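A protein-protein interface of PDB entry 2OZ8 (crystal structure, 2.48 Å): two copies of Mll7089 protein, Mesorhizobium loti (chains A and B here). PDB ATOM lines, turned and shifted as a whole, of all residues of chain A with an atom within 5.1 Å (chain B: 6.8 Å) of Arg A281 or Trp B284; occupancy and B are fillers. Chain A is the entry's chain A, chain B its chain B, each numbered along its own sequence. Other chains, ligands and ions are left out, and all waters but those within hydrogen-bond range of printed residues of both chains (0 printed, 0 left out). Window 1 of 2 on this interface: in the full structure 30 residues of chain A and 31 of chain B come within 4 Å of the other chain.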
ATOM      1  N   VAL A  84     -17.742 -22.068  -3.427  1.00  0.00           N
ATOM      2  CA  VAL A  84     -18.908 -22.918  -3.618  1.00  0.00           C
ATOM      3  C   VAL A  84     -19.280 -23.697  -2.344  1.00  0.00           C
ATOM      4  O   VAL A  84     -20.346 -24.307  -2.275  1.00  0.00           O
ATOM      5  CB  VAL A  84     -18.731 -23.956  -4.821  1.00  0.00           C
ATOM      6  CG1 VAL A  84     -18.559 -23.229  -6.165  1.00  0.00           C
ATOM      7  CG2 VAL A  84     -17.618 -24.942  -4.556  1.00  0.00           C
ATOM      8  N   HIS A  85     -18.408 -23.688  -1.338  1.00  0.00           N
ATOM      9  CA  HIS A  85     -18.755 -24.399  -0.090  1.00  0.00           C
ATOM     10  C   HIS A  85     -19.297 -23.473   0.942  1.00  0.00           C
ATOM     11  O   HIS A  85     -19.884 -23.925   1.906  1.00  0.00           O
ATOM     12  CB  HIS A  85     -17.598 -25.222   0.481  1.00  0.00           C
ATOM     13  CG  HIS A  85     -17.299 -26.434  -0.327  1.00  0.00           C
ATOM     14  ND1 HIS A  85     -16.154 -26.560  -1.067  1.00  0.00           N
ATOM     15  CD2 HIS A  85     -18.018 -27.556  -0.553  1.00  0.00           C
ATOM     16  CE1 HIS A  85     -16.168 -27.721  -1.704  1.00  0.00           C
ATOM     17  NE2 HIS A  85     -17.292 -28.343  -1.412  1.00  0.00           N
ATOM     18  N   ARG A  86     -19.135 -22.176   0.718  1.00  0.00           N
ATOM     19  CA  ARG A  86     -19.542 -21.220   1.715  1.00  0.00           C
ATOM     20  C   ARG A  86     -21.002 -21.404   2.078  1.00  0.00           C
ATOM     21  O   ARG A  86     -21.838 -21.610   1.200  1.00  0.00           O
ATOM     22  CB  ARG A  86     -19.324 -19.796   1.226  1.00  0.00           C
ATOM     23  CG  ARG A  86     -19.505 -18.753   2.340  1.00  0.00           C
ATOM     24  CD  ARG A  86     -18.694 -17.547   1.913  1.00  0.00           C
ATOM     25  NE  ARG A  86     -17.253 -17.747   2.073  1.00  0.00           N
ATOM     26  CZ  ARG A  86     -16.352 -16.876   1.677  1.00  0.00           C
ATOM     27  NH1 ARG A  86     -16.754 -15.772   1.055  1.00  0.00           N
ATOM     28  NH2 ARG A  86     -15.064 -17.107   1.911  1.00  0.00           N
ATOM     29  N   VAL A  87     -21.255 -21.358   3.384  1.00  0.00           N
ATOM     30  CA  VAL A  87     -22.584 -21.257   3.989  1.00  0.00           C
ATOM     31  C   VAL A  87     -22.745 -19.830   4.491  1.00  0.00           C
ATOM     32  O   VAL A  87     -21.977 -19.394   5.363  1.00  0.00           O
ATOM     33  CB  VAL A  87     -22.729 -22.203   5.214  1.00  0.00           C
ATOM     34  CG1 VAL A  87     -24.026 -21.932   5.925  1.00  0.00           C
ATOM     35  CG2 VAL A  87     -22.701 -23.625   4.788  1.00  0.00           C
ATOM     36  N   LEU A 255     -34.567 -21.071  -3.194  1.00  0.00           N
ATOM     37  CA  LEU A 255     -34.106 -22.132  -2.301  1.00  0.00           C
ATOM     38  C   LEU A 255     -34.935 -22.186  -1.039  1.00  0.00           C
ATOM     39  O   LEU A 255     -35.362 -23.276  -0.607  1.00  0.00           O
ATOM     40  CB  LEU A 255     -32.663 -21.908  -1.886  1.00  0.00           C
ATOM     41  CG  LEU A 255     -31.739 -23.127  -1.879  1.00  0.00           C
ATOM     42  CD1 LEU A 255     -30.746 -23.038  -0.722  1.00  0.00           C
ATOM     43  CD2 LEU A 255     -32.456 -24.457  -1.874  1.00  0.00           C
ATOM     44  N   ARG A 259     -37.540 -25.203  -0.070  1.00  0.00           N
ATOM     45  CA  ARG A 259     -37.473 -25.780   1.248  1.00  0.00           C
ATOM     46  C   ARG A 259     -38.831 -25.662   1.976  1.00  0.00           C
ATOM     47  O   ARG A 259     -39.342 -26.659   2.514  1.00  0.00           O
ATOM     48  CB  ARG A 259     -36.324 -25.208   2.063  1.00  0.00           C
ATOM     49  CG  ARG A 259     -36.175 -25.936   3.412  1.00  0.00           C
ATOM     50  CD  ARG A 259     -35.155 -25.338   4.328  1.00  0.00           C
ATOM     51  NE  ARG A 259     -35.406 -23.919   4.487  1.00  0.00           N
ATOM     52  CZ  ARG A 259     -36.264 -23.404   5.347  1.00  0.00           C
ATOM     53  NH1 ARG A 259     -36.937 -24.186   6.162  1.00  0.00           N
ATOM     54  NH2 ARG A 259     -36.425 -22.099   5.412  1.00  0.00           N
ATOM     55  N   THR A 277     -25.180 -24.839  -6.674  1.00  0.00           N
ATOM     56  CA  THR A 277     -25.049 -25.021  -5.242  1.00  0.00           C
ATOM     57  C   THR A 277     -26.399 -25.175  -4.531  1.00  0.00           C
ATOM     58  O   THR A 277     -26.537 -26.041  -3.663  1.00  0.00           O
ATOM     59  CB  THR A 277     -24.284 -23.832  -4.564  1.00  0.00           C
ATOM     60  OG1 THR A 277     -23.057 -23.559  -5.270  1.00  0.00           O
ATOM     61  CG2 THR A 277     -23.991 -24.149  -3.063  1.00  0.00           C
ATOM     62  N   ASP A 278     -27.389 -24.358  -4.878  1.00  0.00           N
ATOM     63  CA  ASP A 278     -28.732 -24.515  -4.280  1.00  0.00           C
ATOM     64  C   ASP A 278     -29.324 -25.897  -4.581  1.00  0.00           C
ATOM     65  O   ASP A 278     -29.948 -26.495  -3.701  1.00  0.00           O
ATOM     66  CB  ASP A 278     -29.734 -23.468  -4.756  1.00  0.00           C
ATOM     67  CG  ASP A 278     -29.253 -22.046  -4.593  1.00  0.00           C
ATOM     68  OD1 ASP A 278     -28.211 -21.818  -3.943  1.00  0.00           O
ATOM     69  OD2 ASP A 278     -29.939 -21.130  -5.132  1.00  0.00           O
ATOM     70  N   VAL A 279     -29.129 -26.375  -5.829  1.00  0.00           N
ATOM     71  CA  VAL A 279     -29.658 -27.669  -6.301  1.00  0.00           C
ATOM     72  C   VAL A 279     -29.065 -28.852  -5.591  1.00  0.00           C
ATOM     73  O   VAL A 279     -29.799 -29.793  -5.227  1.00  0.00           O
ATOM     74  CB  VAL A 279     -29.499 -27.835  -7.826  1.00  0.00           C
ATOM     75  CG1 VAL A 279     -29.843 -29.239  -8.270  1.00  0.00           C
ATOM     76  CG2 VAL A 279     -30.402 -26.831  -8.548  1.00  0.00           C
ATOM     77  N   MET A 280     -27.754 -28.841  -5.377  1.00  0.00           N
ATOM     78  CA  MET A 280     -27.154 -29.926  -4.589  1.00  0.00           C
ATOM     79  C   MET A 280     -27.564 -29.885  -3.112  1.00  0.00           C
ATOM     80  O   MET A 280     -27.691 -30.921  -2.451  1.00  0.00           O
ATOM     81  CB  MET A 280     -25.643 -29.993  -4.762  1.00  0.00           C
ATOM     82  CG  MET A 280     -25.207 -30.218  -6.231  1.00  0.00           C
ATOM     83  SD  MET A 280     -25.739 -31.751  -7.065  1.00  0.00           S
ATOM     84  CE  MET A 280     -24.926 -32.907  -5.955  1.00  0.00           C
ATOM     85  N   ARG A 281     -27.826 -28.703  -2.588  1.00  0.00           N
ATOM     86  CA  ARG A 281     -28.299 -28.625  -1.220  1.00  0.00           C
ATOM     87  C   ARG A 281     -29.771 -29.109  -1.117  1.00  0.00           C
ATOM     88  O   ARG A 281     -30.102 -29.909  -0.214  1.00  0.00           O
ATOM     89  CB  ARG A 281     -28.144 -27.197  -0.674  1.00  0.00           C
ATOM     90  CG  ARG A 281     -26.744 -26.891  -0.320  1.00  0.00           C
ATOM     91  CD  ARG A 281     -26.495 -25.428   0.002  1.00  0.00           C
ATOM     92  NE  ARG A 281     -25.083 -25.287   0.339  1.00  0.00           N
ATOM     93  CZ  ARG A 281     -24.440 -24.142   0.566  1.00  0.00           C
ATOM     94  NH1 ARG A 281     -25.074 -22.965   0.506  1.00  0.00           N
ATOM     95  NH2 ARG A 281     -23.133 -24.193   0.858  1.00  0.00           N
ATOM     96  N   ILE A 282     -30.643 -28.617  -2.010  1.00  0.00           N
ATOM     97  CA  ILE A 282     -32.035 -29.049  -1.988  1.00  0.00           C
ATOM     98  C   ILE A 282     -32.146 -30.516  -2.393  1.00  0.00           C
ATOM     99  O   ILE A 282     -33.033 -31.232  -1.923  1.00  0.00           O
ATOM    100  CB  ILE A 282     -33.007 -28.141  -2.829  1.00  0.00           C
ATOM    101  CG1 ILE A 282     -34.423 -28.307  -2.285  1.00  0.00           C
ATOM    102  CG2 ILE A 282     -33.034 -28.519  -4.290  1.00  0.00           C
ATOM    103  CD1 ILE A 282     -34.627 -27.738  -0.892  1.00  0.00           C
ATOM    104  N   GLY A 283     -31.220 -30.971  -3.239  1.00  0.00           N
ATOM    105  CA  GLY A 283     -31.124 -32.392  -3.575  1.00  0.00           C
ATOM    106  C   GLY A 283     -30.695 -33.310  -2.443  1.00  0.00           C
ATOM    107  O   GLY A 283     -31.089 -34.456  -2.431  1.00  0.00           O
ATOM    108  N   TRP A 284     -29.855 -32.838  -1.519  1.00  0.00           N
ATOM    109  CA  TRP A 284     -29.562 -33.602  -0.293  1.00  0.00           C
ATOM    110  C   TRP A 284     -30.870 -33.728   0.571  1.00  0.00           C
ATOM    111  O   TRP A 284     -31.338 -34.842   0.898  1.00  0.00           O
ATOM    112  CB  TRP A 284     -28.423 -32.954   0.513  1.00  0.00           C
ATOM    113  CG  TRP A 284     -28.384 -33.483   1.882  1.00  0.00           C
ATOM    114  CD1 TRP A 284     -28.056 -34.769   2.256  1.00  0.00           C
ATOM    115  CD2 TRP A 284     -28.789 -32.815   3.070  1.00  0.00           C
ATOM    116  NE1 TRP A 284     -28.211 -34.924   3.589  1.00  0.00           N
ATOM    117  CE2 TRP A 284     -28.671 -33.749   4.133  1.00  0.00           C
ATOM    118  CE3 TRP A 284     -29.247 -31.533   3.350  1.00  0.00           C
ATOM    119  CZ2 TRP A 284     -28.972 -33.428   5.476  1.00  0.00           C
ATOM    120  CZ3 TRP A 284     -29.535 -31.211   4.708  1.00  0.00           C
ATOM    121  CH2 TRP A 284     -29.395 -32.166   5.736  1.00  0.00           C
ATOM    122  N   LEU A 285     -31.437 -32.576   0.931  1.00  0.00           N
ATOM    123  CA  LEU A 285     -32.674 -32.513   1.685  1.00  0.00           C
ATOM    124  C   LEU A 285     -33.766 -33.430   1.062  1.00  0.00           C
ATOM    125  O   LEU A 285     -34.200 -34.366   1.694  1.00  0.00           O
ATOM    126  CB  LEU A 285     -33.136 -31.056   1.866  1.00  0.00           C
ATOM    127  CG  LEU A 285     -34.258 -30.850   2.876  1.00  0.00           C
ATOM    128  CD1 LEU A 285     -33.873 -31.459   4.248  1.00  0.00           C
ATOM    129  CD2 LEU A 285     -34.622 -29.348   3.020  1.00  0.00           C
ATOM    130  N   VAL B  87     -24.337 -37.292  -2.852  1.00  0.00           N
ATOM    131  CA  VAL B  87     -25.643 -37.411  -2.210  1.00  0.00           C
ATOM    132  C   VAL B  87     -26.048 -38.859  -2.440  1.00  0.00           C
ATOM    133  O   VAL B  87     -26.186 -39.297  -3.585  1.00  0.00           O
ATOM    134  CB  VAL B  87     -26.659 -36.440  -2.828  1.00  0.00           C
ATOM    135  CG1 VAL B  87     -28.019 -36.596  -2.167  1.00  0.00           C
ATOM    136  CG2 VAL B  87     -26.155 -35.008  -2.761  1.00  0.00           C
ATOM    137  N   ASP B 278     -21.746 -34.359   6.942  1.00  0.00           N
ATOM    138  CA  ASP B 278     -23.012 -34.230   7.656  1.00  0.00           C
ATOM    139  C   ASP B 278     -23.154 -32.850   8.348  1.00  0.00           C
ATOM    140  O   ASP B 278     -24.226 -32.253   8.298  1.00  0.00           O
ATOM    141  CB  ASP B 278     -23.148 -35.328   8.721  1.00  0.00           C
ATOM    142  CG  ASP B 278     -23.104 -36.746   8.161  1.00  0.00           C
ATOM    143  OD1 ASP B 278     -23.073 -36.929   6.904  1.00  0.00           O
ATOM    144  OD2 ASP B 278     -23.098 -37.683   9.018  1.00  0.00           O
ATOM    145  N   VAL B 279     -22.078 -32.391   9.010  1.00  0.00           N
ATOM    146  CA  VAL B 279     -22.067 -31.141   9.775  1.00  0.00           C
ATOM    147  C   VAL B 279     -22.212 -29.971   8.829  1.00  0.00           C
ATOM    148  O   VAL B 279     -22.956 -29.009   9.113  1.00  0.00           O
ATOM    149  CB  VAL B 279     -20.813 -31.023  10.682  1.00  0.00           C
ATOM    150  CG1 VAL B 279     -20.654 -29.556  11.309  1.00  0.00           C
ATOM    151  CG2 VAL B 279     -20.870 -32.079  11.780  1.00  0.00           C
ATOM    152  N   MET B 280     -21.572 -30.051   7.667  1.00  0.00           N
ATOM    153  CA  MET B 280     -21.798 -28.975   6.701  1.00  0.00           C
ATOM    154  C   MET B 280     -23.194 -29.024   6.084  1.00  0.00           C
ATOM    155  O   MET B 280     -23.716 -27.995   5.714  1.00  0.00           O
ATOM    156  CB  MET B 280     -20.677 -28.826   5.625  1.00  0.00           C
ATOM    157  CG  MET B 280     -19.247 -28.595   6.192  1.00  0.00           C
ATOM    158  SD  MET B 280     -18.961 -27.081   7.114  1.00  0.00           S
ATOM    159  CE  MET B 280     -19.242 -25.911   5.818  1.00  0.00           C
ATOM    160  N   ARG B 281     -23.790 -30.189   5.949  1.00  0.00           N
ATOM    161  CA  ARG B 281     -25.181 -30.224   5.493  1.00  0.00           C
ATOM    162  C   ARG B 281     -26.209 -29.732   6.541  1.00  0.00           C
ATOM    163  O   ARG B 281     -27.071 -28.903   6.218  1.00  0.00           O
ATOM    164  CB  ARG B 281     -25.558 -31.575   4.921  1.00  0.00           C
ATOM    165  CG  ARG B 281     -24.732 -31.884   3.686  1.00  0.00           C
ATOM    166  CD  ARG B 281     -24.705 -33.378   3.368  1.00  0.00           C
ATOM    167  NE  ARG B 281     -24.282 -33.572   1.987  1.00  0.00           N
ATOM    168  CZ  ARG B 281     -24.231 -34.757   1.376  1.00  0.00           C
ATOM    169  NH1 ARG B 281     -24.560 -35.865   2.024  1.00  0.00           N
ATOM    170  NH2 ARG B 281     -23.848 -34.822   0.105  1.00  0.00           N
ATOM    171  N   ILE B 282     -26.122 -30.210   7.779  1.00  0.00           N
ATOM    172  CA  ILE B 282     -26.984 -29.700   8.790  1.00  0.00           C
ATOM    173  C   ILE B 282     -26.648 -28.230   9.118  1.00  0.00           C
ATOM    174  O   ILE B 282     -27.520 -27.442   9.533  1.00  0.00           O
ATOM    175  CB  ILE B 282     -27.048 -30.611  10.039  1.00  0.00           C
ATOM    176  CG1 ILE B 282     -28.393 -30.399  10.773  1.00  0.00           C
ATOM    177  CG2 ILE B 282     -25.882 -30.357  10.997  1.00  0.00           C
ATOM    178  CD1 ILE B 282     -29.532 -31.146  10.135  1.00  0.00           C
ATOM    179  N   GLY B 283     -25.399 -27.837   8.895  1.00  0.00           N
ATOM    180  CA  GLY B 283     -25.042 -26.428   9.068  1.00  0.00           C
ATOM    181  C   GLY B 283     -25.642 -25.481   8.030  1.00  0.00           C
ATOM    182  O   GLY B 283     -25.955 -24.337   8.364  1.00  0.00           O
ATOM    183  N   TRP B 284     -25.783 -25.927   6.779  1.00  0.00           N
ATOM    184  CA  TRP B 284     -26.500 -25.137   5.806  1.00  0.00           C
ATOM    185  C   TRP B 284     -27.984 -24.981   6.255  1.00  0.00           C
ATOM    186  O   TRP B 284     -28.540 -23.871   6.245  1.00  0.00           O
ATOM    187  CB  TRP B 284     -26.413 -25.746   4.394  1.00  0.00           C
ATOM    188  CG  TRP B 284     -27.532 -25.289   3.572  1.00  0.00           C
ATOM    189  CD1 TRP B 284     -27.749 -23.990   3.085  1.00  0.00           C
ATOM    190  CD2 TRP B 284     -28.688 -26.058   3.202  1.00  0.00           C
ATOM    191  NE1 TRP B 284     -28.966 -23.946   2.411  1.00  0.00           N
ATOM    192  CE2 TRP B 284     -29.563 -25.186   2.478  1.00  0.00           C
ATOM    193  CE3 TRP B 284     -29.071 -27.384   3.408  1.00  0.00           C
ATOM    194  CZ2 TRP B 284     -30.768 -25.626   1.947  1.00  0.00           C
ATOM    195  CZ3 TRP B 284     -30.267 -27.836   2.872  1.00  0.00           C
ATOM    196  CH2 TRP B 284     -31.110 -26.954   2.149  1.00  0.00           C
ATOM    197  N   LEU B 285     -28.588 -26.102   6.650  1.00  0.00           N
ATOM    198  CA  LEU B 285     -29.975 -26.171   7.107  1.00  0.00           C
ATOM    199  C   LEU B 285     -30.245 -25.309   8.310  1.00  0.00           C
ATOM    200  O   LEU B 285     -31.146 -24.454   8.255  1.00  0.00           O
ATOM    201  CB  LEU B 285     -30.398 -27.622   7.376  1.00  0.00           C
ATOM    202  CG  LEU B 285     -31.894 -27.860   7.607  1.00  0.00           C
ATOM    203  CD1 LEU B 285     -32.727 -27.373   6.405  1.00  0.00           C
ATOM    204  CD2 LEU B 285     -32.187 -29.325   7.941  1.00  0.00           C
ATOM    205  N   ALA B 286     -29.460 -25.498   9.378  1.00  0.00           N
ATOM    206  CA  ALA B 286     -29.580 -24.672  10.594  1.00  0.00           C
ATOM    207  C   ALA B 286     -29.537 -23.176  10.300  1.00  0.00           C
ATOM    208  O   ALA B 286     -30.236 -22.339  10.953  1.00  0.00           O
ATOM    209  CB  ALA B 286     -28.519 -25.039  11.569  1.00  0.00           C
ATOM    210  N   ALA B 287     -28.705 -22.831   9.324  1.00  0.00           N
ATOM    211  CA  ALA B 287     -28.545 -21.452   8.896  1.00  0.00           C
ATOM    212  C   ALA B 287     -29.824 -20.928   8.232  1.00  0.00           C
ATOM    213  O   ALA B 287     -30.211 -19.823   8.509  1.00  0.00           O
ATOM    214  CB  ALA B 287     -27.353 -21.304   7.959  1.00  0.00           C
ATOM    215  N   GLU B 288     -30.474 -21.722   7.386  1.00  0.00           N
ATOM    216  CA  GLU B 288     -31.694 -21.325   6.745  1.00  0.00           C
ATOM    217  C   GLU B 288     -32.832 -21.061   7.753  1.00  0.00           C
ATOM    218  O   GLU B 288     -33.727 -20.212   7.532  1.00  0.00           O
ATOM    219  CB  GLU B 288     -32.140 -22.423   5.784  1.00  0.00           C
ATOM    220  CG  GLU B 288     -31.228 -22.684   4.612  1.00  0.00           C
ATOM    221  CD  GLU B 288     -31.122 -21.495   3.665  1.00  0.00           C
ATOM    222  OE1 GLU B 288     -31.899 -21.458   2.658  1.00  0.00           O
ATOM    223  OE2 GLU B 288     -30.265 -20.604   3.930  1.00  0.00           O
ATOM    224  N   LEU B 289     -32.760 -21.811   8.850  1.00  0.00           N
ATOM    225  CA  LEU B 289     -33.723 -21.882   9.918  1.00  0.00           C
ATOM    226  C   LEU B 289     -33.427 -20.899  11.055  1.00  0.00           C
ATOM    227  O   LEU B 289     -34.313 -20.633  11.878  1.00  0.00           O
ATOM    228  CB  LEU B 289     -33.724 -23.320  10.468  1.00  0.00           C
ATOM    229  CG  LEU B 289     -34.379 -24.445   9.604  1.00  0.00           C
ATOM    230  CD1 LEU B 289     -34.446 -25.847  10.308  1.00  0.00           C
ATOM    231  CD2 LEU B 289     -35.798 -24.010   9.143  1.00  0.00           C
ATOM    232  N   ILE B 293     -25.468 -23.378  16.357  1.00  0.00           N
ATOM    233  CA  ILE B 293     -24.873 -24.719  16.480  1.00  0.00           C
ATOM    234  C   ILE B 293     -23.620 -24.577  17.312  1.00  0.00           C
ATOM    235  O   ILE B 293     -22.913 -23.571  17.207  1.00  0.00           O
ATOM    236  CB  ILE B 293     -24.454 -25.331  15.095  1.00  0.00           C
ATOM    237  CG1 ILE B 293     -25.678 -25.736  14.262  1.00  0.00           C
ATOM    238  CG2 ILE B 293     -23.449 -26.537  15.287  1.00  0.00           C
ATOM    239  CD1 ILE B 293     -25.329 -26.302  12.863  1.00  0.00           C
ATOM    240  N   LEU B 310     -18.638 -22.360   9.633  1.00  0.00           N
ATOM    241  CA  LEU B 310     -20.057 -22.102   9.826  1.00  0.00           C
ATOM    242  C   LEU B 310     -20.317 -20.762  10.490  1.00  0.00           C
ATOM    243  O   LEU B 310     -19.799 -20.470  11.596  1.00  0.00           O
ATOM    244  CB  LEU B 310     -20.757 -23.220  10.554  1.00  0.00           C
ATOM    245  CG  LEU B 310     -20.792 -24.518   9.701  1.00  0.00           C
ATOM    246  CD1 LEU B 310     -21.207 -25.710  10.534  1.00  0.00           C
ATOM    247  CD2 LEU B 310     -21.664 -24.420   8.465  1.00  0.00           C
ATOM    248  N   GLU B 312     -23.064 -19.774  11.947  1.00  0.00           N
ATOM    249  CA  GLU B 312     -23.879 -19.891  13.171  1.00  0.00           C
ATOM    250  C   GLU B 312     -23.228 -20.683  14.298  1.00  0.00           C
ATOM    251  O   GLU B 312     -23.895 -21.035  15.279  1.00  0.00           O
ATOM    252  CB  GLU B 312     -25.236 -20.526  12.856  1.00  0.00           C
ATOM    253  CG  GLU B 312     -25.207 -22.004  12.614  1.00  0.00           C
ATOM    254  CD  GLU B 312     -24.974 -22.398  11.187  1.00  0.00           C
ATOM    255  OE1 GLU B 312     -24.256 -21.708  10.456  1.00  0.00           O
ATOM    256  OE2 GLU B 312     -25.488 -23.443  10.774  1.00  0.00           O
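Of the printed residues of chain A, Ala B287 touches Val A87 (3.9 Å). Of the printed residues of chain A, Arg B281 touches Trp A284. Ile B293 touches none of the printed residues of chain A. The nearest residue of chain A that does not touch Trp B284 is Val A87 (4.1 Å).
Val A87 touches Gly B283, and with the chains exchanged Gly A283 touches Val B87. Arg A281 touches Trp B284, and with the chains exchanged Trp A284 touches Arg B281. Trp A284 touches Val B87, but with the chains exchanged Val A87 does not touch Trp B284 (4.1 Å). Trp A284 touches its own counterpart, Trp B284. 9 positions are printed for both chains.
Among the printed residues, merely in contact across the chains: Arg A259 with Leu B289 (3.2 Å), Arg A281 with Trp B284 (3.6 Å), Trp A284 with Arg B281 (3.7 Å), Leu A255 with Trp B284 (3.7 Å), Gly A283 with Val B87 (3.8 Å), Arg A259 with Leu B285 (3.8 Å), Arg A259 with Glu B288 (3.8 Å), Trp A284 with Val B87 (3.9 Å), Trp A284 with Trp B284 (3.9 Å), Val A87 with Leu B310 (3.9 Å), Leu A255 with Glu B288 (3.9 Å), Val A87 with Gly B283 (3.9 Å) and Val A87 with Ala B287 (3.9 Å).
Printed residues of chain B that touch a printed residue of chain A: Val B87, Arg B281, Gly B283, Trp B284, Leu B285, Ala B287, Glu B288, Leu B289 and Leu B310. Hydrophobic or aromatic side chains of chain B that line the printed part of chain A: Val B87, Trp B284, Leu B285, Ala B287, Leu B289 and Leu B310. Printed residues of chain A that touch a printed residue of chain B: Val A87, Leu A255, Arg A259, Arg A281, Gly A283 and Trp A284. Hydrophobic or aromatic side chains of chain A that line the printed part of chain B: Val A87, Leu A255 and Trp A284. Among the printed residues, 13 pairs touch across the chains.
O of His A85 is in hydrogen-bond range of NH2 of Arg A281 (3.4 Å). The backbone carbonyl oxygen (O) of Gly B283 sits close to the side-chain carboxylate (OE2) of Glu B312 (2.6 Å). The backbone carbonyl oxygen (O) of Arg A86 lies within hydrogen-bond range of the guanidinium group (NH2) of Arg A281 (2.9 Å).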
